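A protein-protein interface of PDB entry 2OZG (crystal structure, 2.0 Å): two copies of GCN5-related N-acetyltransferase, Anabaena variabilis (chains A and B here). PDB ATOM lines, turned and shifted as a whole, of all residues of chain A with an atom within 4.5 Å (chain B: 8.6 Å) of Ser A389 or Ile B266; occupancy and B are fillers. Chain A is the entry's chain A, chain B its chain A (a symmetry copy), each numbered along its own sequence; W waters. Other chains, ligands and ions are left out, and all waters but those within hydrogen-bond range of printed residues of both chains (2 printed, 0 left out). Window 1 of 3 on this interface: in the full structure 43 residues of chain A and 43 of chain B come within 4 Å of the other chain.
Val A265 touches its own counterpart, Val B265. Of the 12 pairs that touch across the chains among the printed residues, 1 has its exchanged pair printed and touching as well.
Water W2 bridges O of Val B265 (2.8 Å) and NH2 of Arg A285 (3.1 Å). Water W1 lies within hydrogen-bond range of the backbone carbonyl oxygen (O) of Val A265 and the side-chain amide oxygen (OE1) of Gln B283.
Hydrophobic or aromatic side chains of chain A that line the printed part of chain B: Val A265, Leu A359 and Phe A360. Of the 24 printed residues of chain B, 8 touch a printed residue of chain A. Hydrophobic or aromatic side chains of chain B within 4 Å of the printed part of chain A: Val B265, Ile B266, Ala B268 and Leu B271. Among the printed residues, 12 pairs touch across the chains. Among the printed residues, Asp or Glu carboxylates within 4 Å of a Lys or Arg side-chain nitrogen of the other chain: Glu A388 with Arg B363.
Val B265 touches Val A265. CD1 of Ile B266 touches CB of Val A265, 3.8 Å away. Leu A359 touches Ile B266. Ile B266 touches Phe A360. Phe A360 touches Asp B267. Phe A360 touches Ala B268. Phe A360 touches Leu B271. Ser A389 touches Ile B266 (OG to CD1, 3.9 Å).
Of the printed residues of chain B, Ser A389 touches Ile B266. No residue of chain B comes within 4 Å of Pro A390. Of the printed residues of chain A, Ile B266 touches Val A265, Leu A359, Phe A360 and Ser A389. Printed residues of chain A within 4 Å of Ala B268: Phe A360 (3.6 Å). Of the printed residues of chain A, Arg B363 touches Glu A388. The nearest residue of chain B that does not touch Ser A389 is Gln B364 (6.7 Å).
The side-chain carboxylate (OD1) of Asp B267 is in hydrogen-bond range of the indole nitrogen (NE1) of Trp B261 (3.5 Å). OG of Ser B263 is in hydrogen-bond range of OD1 of Asp B267, at 2.7 Å. OG of Ser B264 lies within hydrogen-bond range of N of Ile B266. The backbone NH (N) of Leu B269 lies within hydrogen-bond range of the side-chain carboxylate (OD2) of Asp B267. The backbone NH of Thr B270 sits at hydrogen-bond distance from the side-chain carboxylate of Asp B267 (2.8 Å). N of Thr B361 sits at hydrogen-bond distance from OE1 of Gln B364 (2.9 Å).
NH2 of Arg A285 sits at hydrogen-bond distance from O of Asp B267 (3.0 Å). OG1 of Thr B270 sits at hydrogen-bond distance from NH1 of Arg A285 (3.2 Å). The side-chain carboxylate (OE2) of Glu A388 lies within hydrogen-bond range of the side-chain hydroxyl (OG1) of Thr B361 (2.7 Å). NH2 of Arg B363 is in salt-bridge range of OE1 of Glu A388 (2.9 Å).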
ATOM      1  N   SER A 136      -3.836   9.348  26.703  1.00  0.00           N
ATOM      2  CA  SER A 136      -3.765   8.705  25.397  1.00  0.00           C
ATOM      3  C   SER A 136      -4.477   7.374  25.269  1.00  0.00           C
ATOM      4  O   SER A 136      -4.750   6.705  26.261  1.00  0.00           O
ATOM      5  CB  SER A 136      -2.289   8.501  25.043  1.00  0.00           C
ATOM      6  OG  SER A 136      -1.606   9.755  25.050  1.00  0.00           O
ATOM      7  N   HIS A 179      -1.479   4.458  35.403  1.00  0.00           N
ATOM      8  CA  HIS A 179      -1.839   5.884  35.564  1.00  0.00           C
ATOM      9  C   HIS A 179      -2.771   6.240  34.404  1.00  0.00           C
ATOM     10  O   HIS A 179      -2.402   6.112  33.202  1.00  0.00           O
ATOM     11  CB  HIS A 179      -0.530   6.679  35.576  1.00  0.00           C
ATOM     12  CG  HIS A 179      -0.617   8.106  36.040  1.00  0.00           C
ATOM     13  ND1 HIS A 179      -1.085   8.471  37.282  1.00  0.00           N
ATOM     14  CD2 HIS A 179      -0.135   9.246  35.474  1.00  0.00           C
ATOM     15  CE1 HIS A 179      -0.946   9.774  37.437  1.00  0.00           C
ATOM     16  NE2 HIS A 179      -0.374  10.270  36.355  1.00  0.00           N
ATOM     17  N   VAL A 265       1.021   4.812  24.086  1.00  0.00           N
ATOM     18  CA  VAL A 265       1.728   5.274  22.894  1.00  0.00           C
ATOM     19  C   VAL A 265       3.171   4.779  22.949  1.00  0.00           C
ATOM     20  O   VAL A 265       3.740   4.434  21.932  1.00  0.00           O
ATOM     21  CB  VAL A 265       1.575   6.789  22.744  1.00  0.00           C
ATOM     22  CG1 VAL A 265       2.231   7.262  21.490  1.00  0.00           C
ATOM     23  CG2 VAL A 265       0.060   7.142  22.659  1.00  0.00           C
ATOM     24  N   ARG A 285      -6.348  11.316  21.827  1.00  0.00           N
ATOM     25  CA  ARG A 285      -6.231  11.845  23.156  1.00  0.00           C
ATOM     26  C   ARG A 285      -7.611  12.099  23.707  1.00  0.00           C
ATOM     27  O   ARG A 285      -8.408  12.772  23.125  1.00  0.00           O
ATOM     28  CB  ARG A 285      -5.388  13.099  23.221  1.00  0.00           C
ATOM     29  CG  ARG A 285      -3.951  12.833  22.871  1.00  0.00           C
ATOM     30  CD  ARG A 285      -3.135  14.117  22.805  1.00  0.00           C
ATOM     31  NE  ARG A 285      -1.793  13.790  22.383  1.00  0.00           N
ATOM     32  CZ  ARG A 285      -0.897  14.669  21.969  1.00  0.00           C
ATOM     33  NH1 ARG A 285      -1.176  15.968  21.977  1.00  0.00           N
ATOM     34  NH2 ARG A 285       0.280  14.237  21.521  1.00  0.00           N
ATOM     35  N   LEU A 359       0.322  14.039  31.365  1.00  0.00           N
ATOM     36  CA  LEU A 359       0.470  13.902  29.920  1.00  0.00           C
ATOM     37  C   LEU A 359       1.669  14.727  29.449  1.00  0.00           C
ATOM     38  O   LEU A 359       2.469  14.274  28.605  1.00  0.00           O
ATOM     39  CB  LEU A 359      -0.813  14.410  29.204  1.00  0.00           C
ATOM     40  CG  LEU A 359      -0.772  14.283  27.686  1.00  0.00           C
ATOM     41  CD1 LEU A 359      -0.556  12.863  27.234  1.00  0.00           C
ATOM     42  CD2 LEU A 359      -2.026  14.867  27.056  1.00  0.00           C
ATOM     43  N   PHE A 360       1.712  15.985  29.905  1.00  0.00           N
ATOM     44  CA  PHE A 360       2.808  16.903  29.636  1.00  0.00           C
ATOM     45  C   PHE A 360       3.390  17.380  30.927  1.00  0.00           C
ATOM     46  O   PHE A 360       2.662  17.519  31.936  1.00  0.00           O
ATOM     47  CB  PHE A 360       2.302  18.089  28.790  1.00  0.00           C
ATOM     48  CG  PHE A 360       1.840  17.653  27.426  1.00  0.00           C
ATOM     49  CD1 PHE A 360       2.729  17.084  26.557  1.00  0.00           C
ATOM     50  CD2 PHE A 360       0.518  17.789  27.041  1.00  0.00           C
ATOM     51  CE1 PHE A 360       2.316  16.655  25.277  1.00  0.00           C
ATOM     52  CE2 PHE A 360       0.111  17.377  25.791  1.00  0.00           C
ATOM     53  CZ  PHE A 360       0.992  16.802  24.927  1.00  0.00           C
ATOM     54  N   GLY A 387       5.109  11.015  36.435  1.00  0.00           N
ATOM     55  CA  GLY A 387       4.463   9.736  36.393  1.00  0.00           C
ATOM     56  C   GLY A 387       4.479   9.132  35.004  1.00  0.00           C
ATOM     57  O   GLY A 387       4.864   9.772  34.038  1.00  0.00           O
ATOM     58  N   GLU A 388       4.082   7.885  34.923  1.00  0.00           N
ATOM     59  CA  GLU A 388       4.020   7.187  33.670  1.00  0.00           C
ATOM     60  C   GLU A 388       2.979   7.915  32.791  1.00  0.00           C
ATOM     61  O   GLU A 388       1.975   8.437  33.300  1.00  0.00           O
ATOM     62  CB  GLU A 388       3.683   5.699  33.890  1.00  0.00           C
ATOM     63  CG  GLU A 388       4.776   4.907  34.666  1.00  0.00           C
ATOM     64  CD  GLU A 388       4.521   3.387  34.737  1.00  0.00           C
ATOM     65  OE1 GLU A 388       3.515   2.961  34.132  1.00  0.00           O
ATOM     66  OE2 GLU A 388       5.329   2.637  35.368  1.00  0.00           O
ATOM     67  N   SER A 389       3.256   7.958  31.498  1.00  0.00           N
ATOM     68  CA  SER A 389       2.411   8.614  30.535  1.00  0.00           C
ATOM     69  C   SER A 389       0.991   8.039  30.652  1.00  0.00           C
ATOM     70  O   SER A 389       0.785   6.808  30.578  1.00  0.00           O
ATOM     71  CB  SER A 389       2.957   8.457  29.110  1.00  0.00           C
ATOM     72  OG  SER A 389       2.349   9.413  28.240  1.00  0.00           O
ATOM     73  N   PRO A 390       0.003   8.926  30.825  1.00  0.00           N
ATOM     74  CA  PRO A 390      -1.358   8.414  31.064  1.00  0.00           C
ATOM     75  C   PRO A 390      -2.064   7.796  29.894  1.00  0.00           C
ATOM     76  O   PRO A 390      -2.097   8.371  28.817  1.00  0.00           O
ATOM     77  CB  PRO A 390      -2.090   9.643  31.551  1.00  0.00           C
ATOM     78  CG  PRO A 390      -1.318  10.827  30.913  1.00  0.00           C
ATOM     79  CD  PRO A 390       0.061  10.408  30.796  1.00  0.00           C
ATOM     80  N   TRP A 391      -2.697   6.641  30.111  1.00  0.00           N
ATOM     81  CA  TRP A 391      -3.468   6.052  29.044  1.00  0.00           C
ATOM     82  C   TRP A 391      -4.556   5.173  29.620  1.00  0.00           C
ATOM     83  O   TRP A 391      -4.596   4.950  30.819  1.00  0.00           O
ATOM     84  CB  TRP A 391      -2.520   5.298  28.094  1.00  0.00           C
ATOM     85  CG  TRP A 391      -1.914   4.003  28.708  1.00  0.00           C
ATOM     86  CD1 TRP A 391      -0.866   3.914  29.604  1.00  0.00           C
ATOM     87  CD2 TRP A 391      -2.330   2.635  28.461  1.00  0.00           C
ATOM     88  NE1 TRP A 391      -0.621   2.596  29.903  1.00  0.00           N
ATOM     89  CE2 TRP A 391      -1.484   1.800  29.198  1.00  0.00           C
ATOM     90  CE3 TRP A 391      -3.298   2.045  27.644  1.00  0.00           C
ATOM     91  CZ2 TRP A 391      -1.609   0.422  29.183  1.00  0.00           C
ATOM     92  CZ3 TRP A 391      -3.410   0.678  27.639  1.00  0.00           C
ATOM     93  CH2 TRP A 391      -2.572  -0.114  28.386  1.00  0.00           C
ATOM     94  N   SER B 136      13.146   7.244  21.322  1.00  0.00           N
ATOM     95  CA  SER B 136      12.232   7.318  20.189  1.00  0.00           C
ATOM     96  C   SER B 136      12.541   8.377  19.150  1.00  0.00           C
ATOM     97  O   SER B 136      13.251   9.341  19.421  1.00  0.00           O
ATOM     98  CB  SER B 136      10.821   7.566  20.729  1.00  0.00           C
ATOM     99  OG  SER B 136      10.453   6.525  21.634  1.00  0.00           O
ATOM    100  N   CYS B 138      10.027   9.928  15.791  1.00  0.00           N
ATOM    101  CA  CYS B 138       8.645   9.867  15.316  1.00  0.00           C
ATOM    102  C   CYS B 138       8.446  10.945  14.269  1.00  0.00           C
ATOM    103  O   CYS B 138       8.804  12.112  14.508  1.00  0.00           O
ATOM    104  CB  CYS B 138       7.712  10.157  16.497  1.00  0.00           C
ATOM    105  SG  CYS B 138       6.078   9.896  16.173  1.00  0.00           S
ATOM    106  N   TRP B 140       5.622  12.883  12.323  1.00  0.00           N
ATOM    107  CA  TRP B 140       4.252  13.291  12.346  1.00  0.00           C
ATOM    108  C   TRP B 140       3.855  13.898  11.029  1.00  0.00           C
ATOM    109  O   TRP B 140       4.683  14.448  10.357  1.00  0.00           O
ATOM    110  CB  TRP B 140       4.059  14.364  13.422  1.00  0.00           C
ATOM    111  CG  TRP B 140       4.086  13.791  14.797  1.00  0.00           C
ATOM    112  CD1 TRP B 140       5.179  13.518  15.530  1.00  0.00           C
ATOM    113  CD2 TRP B 140       2.950  13.375  15.578  1.00  0.00           C
ATOM    114  NE1 TRP B 140       4.807  12.989  16.732  1.00  0.00           N
ATOM    115  CE2 TRP B 140       3.444  12.898  16.799  1.00  0.00           C
ATOM    116  CE3 TRP B 140       1.583  13.410  15.381  1.00  0.00           C
ATOM    117  CZ2 TRP B 140       2.605  12.411  17.824  1.00  0.00           C
ATOM    118  CZ3 TRP B 140       0.733  12.949  16.417  1.00  0.00           C
ATOM    119  CH2 TRP B 140       1.271  12.452  17.621  1.00  0.00           C
ATOM    120  N   TRP B 261       6.823  16.664  10.306  1.00  0.00           N
ATOM    121  CA  TRP B 261       7.910  17.068  11.190  1.00  0.00           C
ATOM    122  C   TRP B 261       8.264  15.918  12.117  1.00  0.00           C
ATOM    123  O   TRP B 261       7.415  15.029  12.401  1.00  0.00           O
ATOM    124  CB  TRP B 261       7.543  18.320  11.997  1.00  0.00           C
ATOM    125  CG  TRP B 261       6.589  18.130  13.116  1.00  0.00           C
ATOM    126  CD1 TRP B 261       6.907  18.175  14.434  1.00  0.00           C
ATOM    127  CD2 TRP B 261       5.144  17.909  13.072  1.00  0.00           C
ATOM    128  NE1 TRP B 261       5.781  17.980  15.198  1.00  0.00           N
ATOM    129  CE2 TRP B 261       4.707  17.777  14.397  1.00  0.00           C
ATOM    130  CE3 TRP B 261       4.205  17.765  12.040  1.00  0.00           C
ATOM    131  CZ2 TRP B 261       3.347  17.590  14.729  1.00  0.00           C
ATOM    132  CZ3 TRP B 261       2.894  17.541  12.362  1.00  0.00           C
ATOM    133  CH2 TRP B 261       2.478  17.454  13.677  1.00  0.00           C
ATOM    134  N   SER B 263       9.207  14.746  15.975  1.00  0.00           N
ATOM    135  CA  SER B 263       9.015  15.092  17.307  1.00  0.00           C
ATOM    136  C   SER B 263       9.096  13.817  18.183  1.00  0.00           C
ATOM    137  O   SER B 263       9.632  12.752  17.818  1.00  0.00           O
ATOM    138  CB  SER B 263       7.668  15.784  17.435  1.00  0.00           C
ATOM    139  OG  SER B 263       7.587  16.443  18.647  1.00  0.00           O
ATOM    140  N   SER B 264       8.632  14.011  19.390  1.00  0.00           N
ATOM    141  CA  SER B 264       8.469  12.974  20.333  1.00  0.00           C
ATOM    142  C   SER B 264       7.220  12.176  19.986  1.00  0.00           C
ATOM    143  O   SER B 264       6.298  12.681  19.300  1.00  0.00           O
ATOM    144  CB  SER B 264       8.158  13.616  21.664  1.00  0.00           C
ATOM    145  OG  SER B 264       7.906  12.543  22.543  1.00  0.00           O
ATOM    146  N   VAL B 265       7.113  10.986  20.537  1.00  0.00           N
ATOM    147  CA  VAL B 265       5.912  10.190  20.299  1.00  0.00           C
ATOM    148  C   VAL B 265       4.727  10.860  20.991  1.00  0.00           C
ATOM    149  O   VAL B 265       3.627  10.846  20.473  1.00  0.00           O
ATOM    150  CB  VAL B 265       6.154   8.736  20.706  1.00  0.00           C
ATOM    151  CG1 VAL B 265       4.958   7.898  20.399  1.00  0.00           C
ATOM    152  CG2 VAL B 265       7.358   8.173  19.895  1.00  0.00           C
ATOM    153  N   ILE B 266       4.951  11.465  22.156  1.00  0.00           N
ATOM    154  CA  ILE B 266       3.944  12.259  22.804  1.00  0.00           C
ATOM    155  C   ILE B 266       4.261  13.720  22.471  1.00  0.00           C
ATOM    156  O   ILE B 266       4.741  14.475  23.293  1.00  0.00           O
ATOM    157  CB  ILE B 266       3.912  12.057  24.341  1.00  0.00           C
ATOM    158  CG1 ILE B 266       3.844  10.584  24.664  1.00  0.00           C
ATOM    159  CG2 ILE B 266       2.646  12.747  24.911  1.00  0.00           C
ATOM    160  CD1 ILE B 266       2.524  10.035  24.383  1.00  0.00           C
ATOM    161  N   ASP B 267       3.991  14.103  21.244  1.00  0.00           N
ATOM    162  CA  ASP B 267       4.339  15.424  20.802  1.00  0.00           C
ATOM    163  C   ASP B 267       3.512  16.524  21.497  1.00  0.00           C
ATOM    164  O   ASP B 267       2.300  16.488  21.510  1.00  0.00           O
ATOM    165  CB  ASP B 267       4.171  15.486  19.293  1.00  0.00           C
ATOM    166  CG  ASP B 267       4.104  16.903  18.765  1.00  0.00           C
ATOM    167  OD1 ASP B 267       5.149  17.528  18.599  1.00  0.00           O
ATOM    168  OD2 ASP B 267       2.975  17.364  18.474  1.00  0.00           O
ATOM    169  N   ALA B 268       4.193  17.556  21.968  1.00  0.00           N
ATOM    170  CA  ALA B 268       3.565  18.684  22.636  1.00  0.00           C
ATOM    171  C   ALA B 268       3.062  19.796  21.687  1.00  0.00           C
ATOM    172  O   ALA B 268       2.152  20.564  22.048  1.00  0.00           O
ATOM    173  CB  ALA B 268       4.554  19.267  23.651  1.00  0.00           C
ATOM    174  N   LEU B 269       3.658  19.912  20.494  1.00  0.00           N
ATOM    175  CA  LEU B 269       3.267  20.942  19.552  1.00  0.00           C
ATOM    176  C   LEU B 269       1.797  20.785  19.141  1.00  0.00           C
ATOM    177  O   LEU B 269       1.092  21.772  18.971  1.00  0.00           O
ATOM    178  CB  LEU B 269       4.147  20.906  18.295  1.00  0.00           C
ATOM    179  CG  LEU B 269       5.663  21.172  18.388  1.00  0.00           C
ATOM    180  CD1 LEU B 269       6.213  21.234  16.987  1.00  0.00           C
ATOM    181  CD2 LEU B 269       6.035  22.395  19.118  1.00  0.00           C
ATOM    182  N   THR B 270       1.326  19.552  19.054  1.00  0.00           N
ATOM    183  CA  THR B 270      -0.066  19.270  18.677  1.00  0.00           C
ATOM    184  C   THR B 270      -1.050  19.701  19.779  1.00  0.00           C
ATOM    185  O   THR B 270      -2.255  19.767  19.554  1.00  0.00           O
ATOM    186  CB  THR B 270      -0.251  17.790  18.322  1.00  0.00           C
ATOM    187  OG1 THR B 270       0.333  16.965  19.325  1.00  0.00           O
ATOM    188  CG2 THR B 270       0.410  17.467  16.975  1.00  0.00           C
ATOM    189  N   LEU B 271      -0.535  20.041  20.949  1.00  0.00           N
ATOM    190  CA  LEU B 271      -1.417  20.492  22.031  1.00  0.00           C
ATOM    191  C   LEU B 271      -2.092  21.807  21.618  1.00  0.00           C
ATOM    192  O   LEU B 271      -3.241  22.070  21.971  1.00  0.00           O
ATOM    193  CB  LEU B 271      -0.631  20.651  23.354  1.00  0.00           C
ATOM    194  CG  LEU B 271      -1.415  21.234  24.540  1.00  0.00           C
ATOM    195  CD1 LEU B 271      -2.580  20.353  24.887  1.00  0.00           C
ATOM    196  CD2 LEU B 271      -0.514  21.407  25.706  1.00  0.00           C
ATOM    197  N   ILE B 280       0.691   9.999  13.299  1.00  0.00           N
ATOM    198  CA  ILE B 280       2.033   9.513  13.278  1.00  0.00           C
ATOM    199  C   ILE B 280       2.210   8.740  11.974  1.00  0.00           C
ATOM    200  O   ILE B 280       1.500   7.819  11.722  1.00  0.00           O
ATOM    201  CB  ILE B 280       2.357   8.656  14.535  1.00  0.00           C
ATOM    202  CG1 ILE B 280       2.545   9.591  15.737  1.00  0.00           C
ATOM    203  CG2 ILE B 280       3.576   7.852  14.339  1.00  0.00           C
ATOM    204  CD1 ILE B 280       2.626   8.873  17.095  1.00  0.00           C
ATOM    205  N   GLN B 283       7.476   5.708  13.106  1.00  0.00           N
ATOM    206  CA  GLN B 283       8.279   5.844  14.306  1.00  0.00           C
ATOM    207  C   GLN B 283       9.361   4.787  14.324  1.00  0.00           C
ATOM    208  O   GLN B 283       9.300   3.768  13.609  1.00  0.00           O
ATOM    209  CB  GLN B 283       7.420   5.689  15.533  1.00  0.00           C
ATOM    210  CG  GLN B 283       6.863   4.299  15.660  1.00  0.00           C
ATOM    211  CD  GLN B 283       6.098   4.131  16.913  1.00  0.00           C
ATOM    212  OE1 GLN B 283       6.671   4.174  18.015  1.00  0.00           O
ATOM    213  NE2 GLN B 283       4.790   3.903  16.779  1.00  0.00           N
ATOM    214  N   LEU B 359      13.227   5.418  28.917  1.00  0.00           N
ATOM    215  CA  LEU B 359      12.240   4.986  27.933  1.00  0.00           C
ATOM    216  C   LEU B 359      11.120   4.216  28.636  1.00  0.00           C
ATOM    217  O   LEU B 359       9.924   4.401  28.334  1.00  0.00           O
ATOM    218  CB  LEU B 359      12.909   4.064  26.876  1.00  0.00           C
ATOM    219  CG  LEU B 359      11.965   3.582  25.782  1.00  0.00           C
ATOM    220  CD1 LEU B 359      11.331   4.720  25.026  1.00  0.00           C
ATOM    221  CD2 LEU B 359      12.673   2.628  24.834  1.00  0.00           C
ATOM    222  N   THR B 361       9.958   2.605  32.604  1.00  0.00           N
ATOM    223  CA  THR B 361      10.133   2.757  34.030  1.00  0.00           C
ATOM    224  C   THR B 361      10.595   1.459  34.609  1.00  0.00           C
ATOM    225  O   THR B 361      10.482   0.411  33.969  1.00  0.00           O
ATOM    226  CB  THR B 361       8.812   3.098  34.760  1.00  0.00           C
ATOM    227  OG1 THR B 361       7.855   2.021  34.562  1.00  0.00           O
ATOM    228  CG2 THR B 361       8.244   4.435  34.306  1.00  0.00           C
ATOM    229  N   ARG B 363       9.272  -0.326  36.872  1.00  0.00           N
ATOM    230  CA  ARG B 363       8.118  -1.211  36.934  1.00  0.00           C
ATOM    231  C   ARG B 363       7.880  -1.879  35.587  1.00  0.00           C
ATOM    232  O   ARG B 363       7.631  -3.079  35.520  1.00  0.00           O
ATOM    233  CB  ARG B 363       6.867  -0.399  37.271  1.00  0.00           C
ATOM    234  CG  ARG B 363       5.684  -1.263  37.612  1.00  0.00           C
ATOM    235  CD  ARG B 363       4.394  -0.461  37.684  1.00  0.00           C
ATOM    236  NE  ARG B 363       4.000   0.138  36.405  1.00  0.00           N
ATOM    237  CZ  ARG B 363       3.209  -0.455  35.512  1.00  0.00           C
ATOM    238  NH1 ARG B 363       2.730  -1.673  35.730  1.00  0.00           N
ATOM    239  NH2 ARG B 363       2.898   0.176  34.386  1.00  0.00           N
ATOM    240  N   GLN B 364       7.917  -1.084  34.527  1.00  0.00           N
ATOM    241  CA  GLN B 364       7.752  -1.598  33.153  1.00  0.00           C
ATOM    242  C   GLN B 364       8.874  -2.565  32.755  1.00  0.00           C
ATOM    243  O   GLN B 364       8.645  -3.517  32.056  1.00  0.00           O
ATOM    244  CB  GLN B 364       7.705  -0.441  32.145  1.00  0.00           C
ATOM    245  CG  GLN B 364       6.335   0.304  32.171  1.00  0.00           C
ATOM    246  CD  GLN B 364       6.346   1.516  31.320  1.00  0.00           C
ATOM    247  OE1 GLN B 364       7.314   2.324  31.341  1.00  0.00           O
ATOM    248  NE2 GLN B 364       5.277   1.679  30.531  1.00  0.00           N
ATOM    249  N   GLY B 387      11.985  10.836  34.099  1.00  0.00           N
ATOM    250  CA  GLY B 387      12.298  11.891  33.181  1.00  0.00           C
ATOM    251  C   GLY B 387      11.385  11.888  31.973  1.00  0.00           C
ATOM    252  O   GLY B 387      10.597  10.977  31.774  1.00  0.00           O
ATOM    253  N   GLU B 388      11.481  12.933  31.185  1.00  0.00           N
ATOM    254  CA  GLU B 388      10.696  13.059  29.990  1.00  0.00           C
ATOM    255  C   GLU B 388      11.108  11.905  29.048  1.00  0.00           C
ATOM    256  O   GLU B 388      12.279  11.496  29.023  1.00  0.00           O
ATOM    257  CB  GLU B 388      10.890  14.449  29.353  1.00  0.00           C
ATOM    258  CG  GLU B 388      10.367  15.627  30.228  1.00  0.00           C
ATOM    259  CD  GLU B 388      10.404  16.998  29.523  1.00  0.00           C
ATOM    260  OE1 GLU B 388      10.790  17.005  28.336  1.00  0.00           O
ATOM    261  OE2 GLU B 388      10.028  18.041  30.144  1.00  0.00           O
ATOM    262  N   SER B 389      10.132  11.390  28.318  1.00  0.00           N
ATOM    263  CA  SER B 389      10.327  10.296  27.404  1.00  0.00           C
ATOM    264  C   SER B 389      11.449  10.668  26.423  1.00  0.00           C
ATOM    265  O   SER B 389      11.399  11.727  25.759  1.00  0.00           O
ATOM    266  CB  SER B 389       9.032   9.946  26.662  1.00  0.00           C
ATOM    267  OG  SER B 389       9.136   8.649  26.072  1.00  0.00           O
ATOM    268  N   PRO B 390      12.459   9.795  26.315  1.00  0.00           N
ATOM    269  CA  PRO B 390      13.614  10.169  25.477  1.00  0.00           C
ATOM    270  C   PRO B 390      13.402  10.167  23.993  1.00  0.00           C
ATOM    271  O   PRO B 390      12.873   9.211  23.444  1.00  0.00           O
ATOM    272  CB  PRO B 390      14.653   9.147  25.878  1.00  0.00           C
ATOM    273  CG  PRO B 390      13.824   7.925  26.355  1.00  0.00           C
ATOM    274  CD  PRO B 390      12.600   8.449  26.918  1.00  0.00           C
ATOM    275  N   TRP B 391      13.874  11.213  23.313  1.00  0.00           N
ATOM    276  CA  TRP B 391      13.779  11.217  21.874  1.00  0.00           C
ATOM    277  C   TRP B 391      14.864  12.093  21.289  1.00  0.00           C
ATOM    278  O   TRP B 391      15.571  12.767  22.019  1.00  0.00           O
ATOM    279  CB  TRP B 391      12.361  11.652  21.464  1.00  0.00           C
ATOM    280  CG  TRP B 391      12.062  13.155  21.737  1.00  0.00           C
ATOM    281  CD1 TRP B 391      11.742  13.737  22.949  1.00  0.00           C
ATOM    282  CD2 TRP B 391      12.059  14.241  20.774  1.00  0.00           C
ATOM    283  NE1 TRP B 391      11.542  15.085  22.780  1.00  0.00           N
ATOM    284  CE2 TRP B 391      11.705  15.408  21.459  1.00  0.00           C
ATOM    285  CE3 TRP B 391      12.268  14.318  19.395  1.00  0.00           C
ATOM    286  CZ2 TRP B 391      11.606  16.635  20.826  1.00  0.00           C
ATOM    287  CZ3 TRP B 391      12.165  15.540  18.782  1.00  0.00           C
ATOM    288  CH2 TRP B 391      11.829  16.671  19.485  1.00  0.00           C
HETATM  289  O   HOH W   1       6.202   3.895  20.800  1.00  0.00           O
HETATM  290  O   HOH W   2       0.926  11.223  20.912  1.00  0.00           O
